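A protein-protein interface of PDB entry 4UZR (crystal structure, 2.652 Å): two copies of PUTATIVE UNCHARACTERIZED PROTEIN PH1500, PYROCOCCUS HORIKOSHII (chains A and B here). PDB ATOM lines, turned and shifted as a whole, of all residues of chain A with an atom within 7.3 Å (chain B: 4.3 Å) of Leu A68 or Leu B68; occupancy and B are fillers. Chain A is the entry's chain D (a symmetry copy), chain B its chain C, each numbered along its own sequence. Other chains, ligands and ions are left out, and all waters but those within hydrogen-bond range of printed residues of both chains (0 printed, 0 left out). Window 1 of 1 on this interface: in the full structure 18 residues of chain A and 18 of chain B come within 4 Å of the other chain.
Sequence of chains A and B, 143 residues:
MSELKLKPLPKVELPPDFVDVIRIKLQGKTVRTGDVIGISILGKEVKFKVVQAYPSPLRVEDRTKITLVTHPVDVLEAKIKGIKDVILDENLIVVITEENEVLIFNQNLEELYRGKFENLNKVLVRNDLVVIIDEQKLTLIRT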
ATOM      1  N   LEU A   4      17.154   0.220   2.726  1.00  0.00           N
ATOM      2  CA  LEU A   4      16.029  -0.462   3.358  1.00  0.00           C
ATOM      3  C   LEU A   4      15.384   0.420   4.423  1.00  0.00           C
ATOM      4  O   LEU A   4      15.997   0.747   5.441  1.00  0.00           O
ATOM      5  CB  LEU A   4      16.466  -1.781   3.991  1.00  0.00           C
ATOM      6  CG  LEU A   4      16.050  -3.058   3.269  1.00  0.00           C
ATOM      7  CD1 LEU A   4      16.386  -4.275   4.116  1.00  0.00           C
ATOM      8  CD2 LEU A   4      14.567  -3.015   2.954  1.00  0.00           C
ATOM      9  N   LYS A   5      14.132   0.789   4.178  1.00  0.00           N
ATOM     10  CA  LYS A   5      13.341   1.544   5.134  1.00  0.00           C
ATOM     11  C   LYS A   5      12.317   0.614   5.774  1.00  0.00           C
ATOM     12  O   LYS A   5      11.336   0.206   5.130  1.00  0.00           O
ATOM     13  CB  LYS A   5      12.652   2.725   4.444  1.00  0.00           C
ATOM     14  CG  LYS A   5      13.630   3.787   3.940  1.00  0.00           C
ATOM     15  CD  LYS A   5      12.923   4.953   3.262  1.00  0.00           C
ATOM     16  CE  LYS A   5      13.915   6.041   2.864  1.00  0.00           C
ATOM     17  NZ  LYS A   5      13.404   6.913   1.768  1.00  0.00           N
ATOM     18  N   LEU A   6      12.571   0.294   7.045  1.00  0.00           N
ATOM     19  CA  LEU A   6      11.793  -0.675   7.811  1.00  0.00           C
ATOM     20  C   LEU A   6      10.995  -0.015   8.935  1.00  0.00           C
ATOM     21  O   LEU A   6      11.408   0.998   9.494  1.00  0.00           O
ATOM     22  CB  LEU A   6      12.727  -1.709   8.439  1.00  0.00           C
ATOM     23  CG  LEU A   6      13.630  -2.522   7.520  1.00  0.00           C
ATOM     24  CD1 LEU A   6      14.611  -3.350   8.344  1.00  0.00           C
ATOM     25  CD2 LEU A   6      12.781  -3.413   6.637  1.00  0.00           C
ATOM     26  N   LYS A   7       9.863  -0.617   9.279  1.00  0.00           N
ATOM     27  CA  LYS A   7       9.026  -0.130  10.368  1.00  0.00           C
ATOM     28  C   LYS A   7       8.659  -1.270  11.308  1.00  0.00           C
ATOM     29  O   LYS A   7       8.035  -2.246  10.888  1.00  0.00           O
ATOM     30  CB  LYS A   7       7.757   0.513   9.808  1.00  0.00           C
ATOM     31  CG  LYS A   7       6.735   0.913  10.856  1.00  0.00           C
ATOM     32  CD  LYS A   7       5.345   1.034  10.240  1.00  0.00           C
ATOM     33  CE  LYS A   7       4.334   1.580  11.242  1.00  0.00           C
ATOM     34  NZ  LYS A   7       2.961   1.727  10.668  1.00  0.00           N
ATOM     35  N   PRO A   8       9.039  -1.149  12.590  1.00  0.00           N
ATOM     36  CA  PRO A   8       8.676  -2.177  13.570  1.00  0.00           C
ATOM     37  C   PRO A   8       7.167  -2.198  13.805  1.00  0.00           C
ATOM     38  O   PRO A   8       6.526  -1.148  13.785  1.00  0.00           O
ATOM     39  CB  PRO A   8       9.417  -1.735  14.836  1.00  0.00           C
ATOM     40  CG  PRO A   8       9.703  -0.283  14.640  1.00  0.00           C
ATOM     41  CD  PRO A   8       9.891  -0.096  13.169  1.00  0.00           C
ATOM     42  N   LEU A   9       6.609  -3.389  13.993  1.00  0.00           N
ATOM     43  CA  LEU A   9       5.172  -3.551  14.162  1.00  0.00           C
ATOM     44  C   LEU A   9       4.842  -4.343  15.425  1.00  0.00           C
ATOM     45  O   LEU A   9       5.025  -5.559  15.458  1.00  0.00           O
ATOM     46  CB  LEU A   9       4.562  -4.259  12.947  1.00  0.00           C
ATOM     47  CG  LEU A   9       4.732  -3.654  11.552  1.00  0.00           C
ATOM     48  CD1 LEU A   9       4.126  -4.575  10.510  1.00  0.00           C
ATOM     49  CD2 LEU A   9       4.091  -2.279  11.477  1.00  0.00           C
ATOM     50  N   PRO A  10       4.357  -3.657  16.471  1.00  0.00           N
ATOM     51  CA  PRO A  10       4.203  -2.203  16.522  1.00  0.00           C
ATOM     52  C   PRO A  10       5.324  -1.556  17.328  1.00  0.00           C
ATOM     53  O   PRO A  10       5.288  -0.347  17.569  1.00  0.00           O
ATOM     54  CB  PRO A  10       2.890  -2.043  17.278  1.00  0.00           C
ATOM     55  CG  PRO A  10       2.933  -3.167  18.275  1.00  0.00           C
ATOM     56  CD  PRO A  10       3.667  -4.311  17.598  1.00  0.00           C
ATOM     57  N   LYS A  11       6.296  -2.357  17.752  1.00  0.00           N
ATOM     58  CA  LYS A  11       7.364  -1.869  18.614  1.00  0.00           C
ATOM     59  C   LYS A  11       8.571  -2.796  18.582  1.00  0.00           C
ATOM     60  O   LYS A  11       8.467  -3.953  18.169  1.00  0.00           O
ATOM     61  CB  LYS A  11       6.878  -1.718  20.055  1.00  0.00           C
ATOM     62  CG  LYS A  11       6.441  -3.014  20.704  1.00  0.00           C
ATOM     63  CD  LYS A  11       6.021  -2.781  22.142  1.00  0.00           C
ATOM     64  CE  LYS A  11       5.591  -4.074  22.807  1.00  0.00           C
ATOM     65  NZ  LYS A  11       5.187  -3.841  24.218  1.00  0.00           N
ATOM     66  N   VAL A  12       9.715  -2.271  19.011  1.00  0.00           N
ATOM     67  CA  VAL A  12      10.941  -3.055  19.104  1.00  0.00           C
ATOM     68  C   VAL A  12      11.777  -2.675  20.326  1.00  0.00           C
ATOM     69  O   VAL A  12      12.054  -1.500  20.563  1.00  0.00           O
ATOM     70  CB  VAL A  12      11.789  -2.926  17.817  1.00  0.00           C
ATOM     71  CG1 VAL A  12      12.037  -1.459  17.467  1.00  0.00           C
ATOM     72  CG2 VAL A  12      13.093  -3.703  17.948  1.00  0.00           C
ATOM     73  N   GLU A  13      12.154  -3.677  21.115  1.00  0.00           N
ATOM     74  CA  GLU A  13      13.126  -3.484  22.182  1.00  0.00           C
ATOM     75  C   GLU A  13      14.510  -3.441  21.546  1.00  0.00           C
ATOM     76  O   GLU A  13      14.904  -4.368  20.838  1.00  0.00           O
ATOM     77  CB  GLU A  13      13.034  -4.616  23.207  1.00  0.00           C
ATOM     78  CG  GLU A  13      14.051  -4.527  24.333  1.00  0.00           C
ATOM     79  CD  GLU A  13      13.949  -5.687  25.306  1.00  0.00           C
ATOM     80  OE1 GLU A  13      12.974  -6.463  25.206  1.00  0.00           O
ATOM     81  OE2 GLU A  13      14.847  -5.827  26.164  1.00  0.00           O
ATOM     82  N   LEU A  14      15.244  -2.361  21.792  1.00  0.00           N
ATOM     83  CA  LEU A  14      16.481  -2.094  21.064  1.00  0.00           C
ATOM     84  C   LEU A  14      17.754  -2.437  21.835  1.00  0.00           C
ATOM     85  O   LEU A  14      17.977  -1.936  22.938  1.00  0.00           O
ATOM     86  CB  LEU A  14      16.519  -0.633  20.604  1.00  0.00           C
ATOM     87  CG  LEU A  14      15.535  -0.249  19.499  1.00  0.00           C
ATOM     88  CD1 LEU A  14      15.515   1.257  19.309  1.00  0.00           C
ATOM     89  CD2 LEU A  14      15.898  -0.947  18.195  1.00  0.00           C
ATOM     90  N   PHE A  18      22.320  -1.839  17.155  1.00  0.00           N
ATOM     91  CA  PHE A  18      21.209  -2.577  16.567  1.00  0.00           C
ATOM     92  C   PHE A  18      21.318  -2.672  15.041  1.00  0.00           C
ATOM     93  O   PHE A  18      20.757  -3.583  14.422  1.00  0.00           O
ATOM     94  CB  PHE A  18      19.891  -1.929  17.004  1.00  0.00           C
ATOM     95  CG  PHE A  18      18.679  -2.474  16.315  1.00  0.00           C
ATOM     96  CD1 PHE A  18      18.208  -3.738  16.615  1.00  0.00           C
ATOM     97  CD2 PHE A  18      17.982  -1.706  15.404  1.00  0.00           C
ATOM     98  CE1 PHE A  18      17.082  -4.237  15.995  1.00  0.00           C
ATOM     99  CE2 PHE A  18      16.852  -2.199  14.781  1.00  0.00           C
ATOM    100  CZ  PHE A  18      16.399  -3.465  15.083  1.00  0.00           C
ATOM    101  N   ILE A  22      20.736  -6.008  12.780  1.00  0.00           N
ATOM    102  CA  ILE A  22      19.839  -6.097  11.631  1.00  0.00           C
ATOM    103  C   ILE A  22      20.578  -6.550  10.376  1.00  0.00           C
ATOM    104  O   ILE A  22      20.087  -7.401   9.632  1.00  0.00           O
ATOM    105  CB  ILE A  22      19.120  -4.761  11.362  1.00  0.00           C
ATOM    106  CG1 ILE A  22      18.015  -4.558  12.387  1.00  0.00           C
ATOM    107  CG2 ILE A  22      18.489  -4.753   9.984  1.00  0.00           C
ATOM    108  CD1 ILE A  22      16.920  -5.605  12.309  1.00  0.00           C
ATOM    109  N   PHE A  48       8.655  -6.564  10.920  1.00  0.00           N
ATOM    110  CA  PHE A  48       9.053  -5.320  10.278  1.00  0.00           C
ATOM    111  C   PHE A  48       8.395  -5.217   8.914  1.00  0.00           C
ATOM    112  O   PHE A  48       8.524  -6.116   8.091  1.00  0.00           O
ATOM    113  CB  PHE A  48      10.571  -5.264  10.094  1.00  0.00           C
ATOM    114  CG  PHE A  48      11.337  -5.128  11.372  1.00  0.00           C
ATOM    115  CD1 PHE A  48      11.700  -6.250  12.098  1.00  0.00           C
ATOM    116  CD2 PHE A  48      11.716  -3.880  11.836  1.00  0.00           C
ATOM    117  CE1 PHE A  48      12.417  -6.128  13.274  1.00  0.00           C
ATOM    118  CE2 PHE A  48      12.432  -3.751  13.012  1.00  0.00           C
ATOM    119  CZ  PHE A  48      12.783  -4.877  13.731  1.00  0.00           C
ATOM    120  N   ILE A  66      20.442   0.908   6.087  1.00  0.00           N
ATOM    121  CA  ILE A  66      19.213   0.530   6.774  1.00  0.00           C
ATOM    122  C   ILE A  66      18.743   1.623   7.728  1.00  0.00           C
ATOM    123  O   ILE A  66      19.501   2.093   8.579  1.00  0.00           O
ATOM    124  CB  ILE A  66      19.397  -0.785   7.546  1.00  0.00           C
ATOM    125  CG1 ILE A  66      19.861  -1.887   6.590  1.00  0.00           C
ATOM    126  CG2 ILE A  66      18.103  -1.178   8.247  1.00  0.00           C
ATOM    127  CD1 ILE A  66      20.172  -3.197   7.263  1.00  0.00           C
ATOM    128  N   THR A  67      17.483   2.023   7.583  1.00  0.00           N
ATOM    129  CA  THR A  67      16.909   3.051   8.440  1.00  0.00           C
ATOM    130  C   THR A  67      15.580   2.603   9.030  1.00  0.00           C
ATOM    131  O   THR A  67      14.870   1.787   8.443  1.00  0.00           O
ATOM    132  CB  THR A  67      16.685   4.370   7.673  1.00  0.00           C
ATOM    133  OG1 THR A  67      15.754   4.155   6.607  1.00  0.00           O
ATOM    134  CG2 THR A  67      17.990   4.889   7.098  1.00  0.00           C
ATOM    135  N   LEU A  68      15.247   3.147  10.197  1.00  0.00           N
ATOM    136  CA  LEU A  68      13.979   2.845  10.846  1.00  0.00           C
ATOM    137  C   LEU A  68      12.941   3.917  10.539  1.00  0.00           C
ATOM    138  O   LEU A  68      13.236   5.112  10.579  1.00  0.00           O
ATOM    139  CB  LEU A  68      14.162   2.701  12.358  1.00  0.00           C
ATOM    140  CG  LEU A  68      14.922   1.463  12.837  1.00  0.00           C
ATOM    141  CD1 LEU A  68      14.997   1.440  14.352  1.00  0.00           C
ATOM    142  CD2 LEU A  68      14.237   0.203  12.324  1.00  0.00           C
ATOM    143  N   VAL A  69      11.737   3.470  10.201  1.00  0.00           N
ATOM    144  CA  VAL A  69      10.598   4.347   9.961  1.00  0.00           C
ATOM    145  C   VAL A  69       9.758   4.434  11.233  1.00  0.00           C
ATOM    146  O   VAL A  69       9.534   3.423  11.897  1.00  0.00           O
ATOM    147  CB  VAL A  69       9.754   3.825   8.769  1.00  0.00           C
ATOM    148  CG1 VAL A  69       8.375   4.450   8.750  1.00  0.00           C
ATOM    149  CG2 VAL A  69      10.481   4.081   7.459  1.00  0.00           C
ATOM    150  N   THR A  70       9.319   5.640  11.591  1.00  0.00           N
ATOM    151  CA  THR A  70       8.663   5.851  12.883  1.00  0.00           C
ATOM    152  C   THR A  70       7.209   6.330  12.826  1.00  0.00           C
ATOM    153  O   THR A  70       6.573   6.491  13.868  1.00  0.00           O
ATOM    154  CB  THR A  70       9.447   6.849  13.760  1.00  0.00           C
ATOM    155  OG1 THR A  70       9.525   8.119  13.100  1.00  0.00           O
ATOM    156  CG2 THR A  70      10.842   6.333  14.043  1.00  0.00           C
ATOM    157  N   HIS A  71       6.682   6.566  11.628  1.00  0.00           N
ATOM    158  CA  HIS A  71       5.324   7.095  11.519  1.00  0.00           C
ATOM    159  C   HIS A  71       4.245   6.059  11.841  1.00  0.00           C
ATOM    160  O   HIS A  71       4.257   4.955  11.304  1.00  0.00           O
ATOM    161  CB  HIS A  71       5.075   7.758  10.156  1.00  0.00           C
ATOM    162  CG  HIS A  71       5.296   6.859   8.980  1.00  0.00           C
ATOM    163  ND1 HIS A  71       4.754   5.593   8.892  1.00  0.00           N
ATOM    164  CD2 HIS A  71       5.971   7.055   7.821  1.00  0.00           C
ATOM    165  CE1 HIS A  71       5.104   5.042   7.742  1.00  0.00           C
ATOM    166  NE2 HIS A  71       5.843   5.915   7.073  1.00  0.00           N
ATOM    167  N   LEU B   6       9.382   4.864  24.166  1.00  0.00           N
ATOM    168  CA  LEU B   6       9.591   6.189  23.596  1.00  0.00           C
ATOM    169  C   LEU B   6       9.102   6.279  22.152  1.00  0.00           C
ATOM    170  O   LEU B   6       8.954   5.267  21.468  1.00  0.00           O
ATOM    171  CB  LEU B   6      11.082   6.516  23.588  1.00  0.00           C
ATOM    172  CG  LEU B   6      11.891   6.342  24.868  1.00  0.00           C
ATOM    173  CD1 LEU B   6      13.365   6.470  24.539  1.00  0.00           C
ATOM    174  CD2 LEU B   6      11.476   7.365  25.907  1.00  0.00           C
ATOM    175  N   PRO B   8       9.431   9.359  18.656  1.00  0.00           N
ATOM    176  CA  PRO B   8       9.811  10.705  18.221  1.00  0.00           C
ATOM    177  C   PRO B   8       8.572  11.563  18.004  1.00  0.00           C
ATOM    178  O   PRO B   8       7.538  11.041  17.590  1.00  0.00           O
ATOM    179  CB  PRO B   8      10.519  10.451  16.888  1.00  0.00           C
ATOM    180  CG  PRO B   8       9.898   9.198  16.378  1.00  0.00           C
ATOM    181  CD  PRO B   8       9.607   8.358  17.591  1.00  0.00           C
ATOM    182  N   GLU B  13      12.825   9.598   9.934  1.00  0.00           N
ATOM    183  CA  GLU B  13      13.530   8.335   9.789  1.00  0.00           C
ATOM    184  C   GLU B  13      14.752   8.333  10.699  1.00  0.00           C
ATOM    185  O   GLU B  13      15.505   9.306  10.745  1.00  0.00           O
ATOM    186  CB  GLU B  13      13.936   8.119   8.332  1.00  0.00           C
ATOM    187  CG  GLU B  13      12.751   8.017   7.381  1.00  0.00           C
ATOM    188  CD  GLU B  13      13.173   7.832   5.939  1.00  0.00           C
ATOM    189  OE1 GLU B  13      14.371   7.575   5.696  1.00  0.00           O
ATOM    190  OE2 GLU B  13      12.305   7.948   5.049  1.00  0.00           O
ATOM    191  N   LEU B  14      14.942   7.239  11.426  1.00  0.00           N
ATOM    192  CA  LEU B  14      16.024   7.158  12.396  1.00  0.00           C
ATOM    193  C   LEU B  14      17.063   6.120  12.006  1.00  0.00           C
ATOM    194  O   LEU B  14      16.727   5.083  11.439  1.00  0.00           O
ATOM    195  CB  LEU B  14      15.463   6.808  13.775  1.00  0.00           C
ATOM    196  CG  LEU B  14      14.429   7.761  14.371  1.00  0.00           C
ATOM    197  CD1 LEU B  14      13.883   7.201  15.675  1.00  0.00           C
ATOM    198  CD2 LEU B  14      15.033   9.137  14.590  1.00  0.00           C
ATOM    199  N   PRO B  16      19.291   3.055  13.096  1.00  0.00           N
ATOM    200  CA  PRO B  16      18.879   2.019  14.051  1.00  0.00           C
ATOM    201  C   PRO B  16      19.625   2.044  15.394  1.00  0.00           C
ATOM    202  O   PRO B  16      19.145   1.435  16.350  1.00  0.00           O
ATOM    203  CB  PRO B  16      19.122   0.702  13.292  1.00  0.00           C
ATOM    204  CG  PRO B  16      19.661   1.075  11.946  1.00  0.00           C
ATOM    205  CD  PRO B  16      20.043   2.512  11.956  1.00  0.00           C
ATOM    206  N   PHE B  18      20.293   4.801  17.286  1.00  0.00           N
ATOM    207  CA  PHE B  18      20.003   6.046  18.018  1.00  0.00           C
ATOM    208  C   PHE B  18      19.807   5.847  19.530  1.00  0.00           C
ATOM    209  O   PHE B  18      20.081   6.745  20.349  1.00  0.00           O
ATOM    210  CB  PHE B  18      18.772   6.732  17.413  1.00  0.00           C
ATOM    211  CG  PHE B  18      17.469   6.053  17.747  1.00  0.00           C
ATOM    212  CD1 PHE B  18      17.074   4.912  17.070  1.00  0.00           C
ATOM    213  CD2 PHE B  18      16.641   6.555  18.736  1.00  0.00           C
ATOM    214  CE1 PHE B  18      15.879   4.282  17.373  1.00  0.00           C
ATOM    215  CE2 PHE B  18      15.449   5.932  19.045  1.00  0.00           C
ATOM    216  CZ  PHE B  18      15.067   4.792  18.362  1.00  0.00           C
ATOM    217  N   THR B  67      12.458   0.870  24.402  1.00  0.00           N
ATOM    218  CA  THR B  67      11.652   0.387  23.284  1.00  0.00           C
ATOM    219  C   THR B  67      11.170   1.509  22.361  1.00  0.00           C
ATOM    220  O   THR B  67      10.678   2.539  22.825  1.00  0.00           O
ATOM    221  CB  THR B  67      10.419  -0.387  23.799  1.00  0.00           C
ATOM    222  OG1 THR B  67      10.846  -1.529  24.552  1.00  0.00           O
ATOM    223  CG2 THR B  67       9.544  -0.844  22.645  1.00  0.00           C
ATOM    224  N   LEU B  68      11.321   1.300  21.054  1.00  0.00           N
ATOM    225  CA  LEU B  68      10.777   2.214  20.050  1.00  0.00           C
ATOM    226  C   LEU B  68       9.329   1.851  19.727  1.00  0.00           C
ATOM    227  O   LEU B  68       9.022   0.701  19.418  1.00  0.00           O
ATOM    228  CB  LEU B  68      11.610   2.190  18.767  1.00  0.00           C
ATOM    229  CG  LEU B  68      10.997   2.964  17.594  1.00  0.00           C
ATOM    230  CD1 LEU B  68      10.820   4.442  17.934  1.00  0.00           C
ATOM    231  CD2 LEU B  68      11.813   2.790  16.322  1.00  0.00           C
ATOM    232  N   VAL B  69       8.446   2.839  19.804  1.00  0.00           N
ATOM    233  CA  VAL B  69       7.024   2.625  19.559  1.00  0.00           C
ATOM    234  C   VAL B  69       6.548   3.281  18.260  1.00  0.00           C
ATOM    235  O   VAL B  69       6.893   4.427  17.966  1.00  0.00           O
ATOM    236  CB  VAL B  69       6.193   3.139  20.750  1.00  0.00           C
ATOM    237  CG1 VAL B  69       4.741   3.325  20.366  1.00  0.00           C
ATOM    238  CG2 VAL B  69       6.334   2.191  21.934  1.00  0.00           C
ATOM    239  N   THR B  70       5.777   2.533  17.474  1.00  0.00           N
ATOM    240  CA  THR B  70       5.233   3.035  16.213  1.00  0.00           C
ATOM    241  C   THR B  70       3.715   3.221  16.241  1.00  0.00           C
ATOM    242  O   THR B  70       3.096   3.427  15.201  1.00  0.00           O
ATOM    243  CB  THR B  70       5.614   2.148  15.021  1.00  0.00           C
ATOM    244  OG1 THR B  70       5.230   0.793  15.280  1.00  0.00           O
ATOM    245  CG2 THR B  70       7.112   2.233  14.765  1.00  0.00           C
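The backbone carbonyl oxygen (O) of Leu B14 sits at hydrogen-bond distance from the backbone NH (N) of Leu A68, at 2.7 Å.
The side-chain hydroxyl (OG1) of Thr B70 sits at hydrogen-bond distance from the backbone carbonyl oxygen (O) of Pro A8, 2.8 Å away.
The side-chain hydroxyl (OG1) of Thr B70 lies within hydrogen-bond range of the backbone carbonyl oxygen (O) of Pro A10.
The backbone NH of Leu B68 lies within hydrogen-bond range of the backbone carbonyl oxygen of Val A12 (2.9 Å).
The side-chain amino group (NZ) of Lys A5 is in salt-bridge range of the side-chain carboxylate (OE2) of Glu B13 (3.6 Å).
Printed residues of chain B within 4 Å of Leu A68: Glu B13, Leu B14, Pro B16 and Leu B68.
Printed residues of chain A within 4 Å of Leu B68: Lys A11, Val A12 and Leu A68.
Of the printed residues of chain A, Pro B16 touches Phe A18, Ile A66 and Leu A68.
Printed residues of chain A within 4 Å of Pro B8: Thr A70.
Of the printed residues of chain B, Thr A70 touches Pro B8 (3.5 Å) and Leu B14 (3.6 Å).
Of the printed residues of chain A, Val B69 touches Pro A10.
Phe A48 touches none of the printed residues of chain B.
Leu A9 touches none of the printed residues of chain B.
The nearest printed residue of chain A that does not touch Leu B68 is Leu A14 (4.1 Å).
The nearest printed residue of chain A that does not touch Leu B14 is Ile A66 (5.0 Å).
The backbone carbonyl oxygen of Leu A4 lies within hydrogen-bond range of the backbone NH of Thr A67 (2.9 Å).
O of Thr A67 lies within hydrogen-bond range of N of Leu A6 (3.1 Å).
The backbone NH (N) of Val A69 is in hydrogen-bond range of the backbone carbonyl oxygen (O) of Leu A6, at 2.6 Å.
The backbone carbonyl oxygen (O) of Thr B67 sits at hydrogen-bond distance from the backbone NH (N) of Leu B6.
The backbone carbonyl oxygen (O) of Leu B6 sits at hydrogen-bond distance from the backbone NH (N) of Val B69, at 3.0 Å.
Of the 10 printed residues of chain B, 9 touch a printed residue of chain A.
Printed residues of chain A that touch a printed residue of chain B: Lys A5, Pro A8, Pro A10, Lys A11, Val A12, Glu A13, Leu A14, Phe A18, Ile A66, Thr A67, Leu A68, Val A69 and Thr A70.
Val B69 touches Pro A10 (C to O, 3.9 Å).
Lys A11 touches Thr B67 (CB to CG2, 3.8 Å).
CA of Lys A11 touches O of Leu B68, 3.2 Å away.
Glu A13 touches Thr B67.
Pro B16 touches Phe A18 (CB to CD2, 3.4 Å).
Glu B13 touches Thr A67.
Pro B16 touches Leu A68 (CA to CD1, 3.9 Å).
CD2 of Leu B68 touches CD1 of Leu A68 (3.98 Å).
O of Val A69 touches CG2 of Thr B70 (3.9 Å).
Thr A70 touches Pro B8.
Glu A13 touches Thr B67, and with the chains exchanged Thr A67 touches Glu B13.
Leu A14 touches Phe B18, but with the chains exchanged Phe A18 does not touch Leu B14 (8.0 Å).
Leu A68 touches Glu B13, but with the chains exchanged Glu A13 does not touch Leu B68 (5.0 Å).
Thr A70 touches Leu B14, but with the chains exchanged Leu A14 does not touch Thr B70 (9.6 Å).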
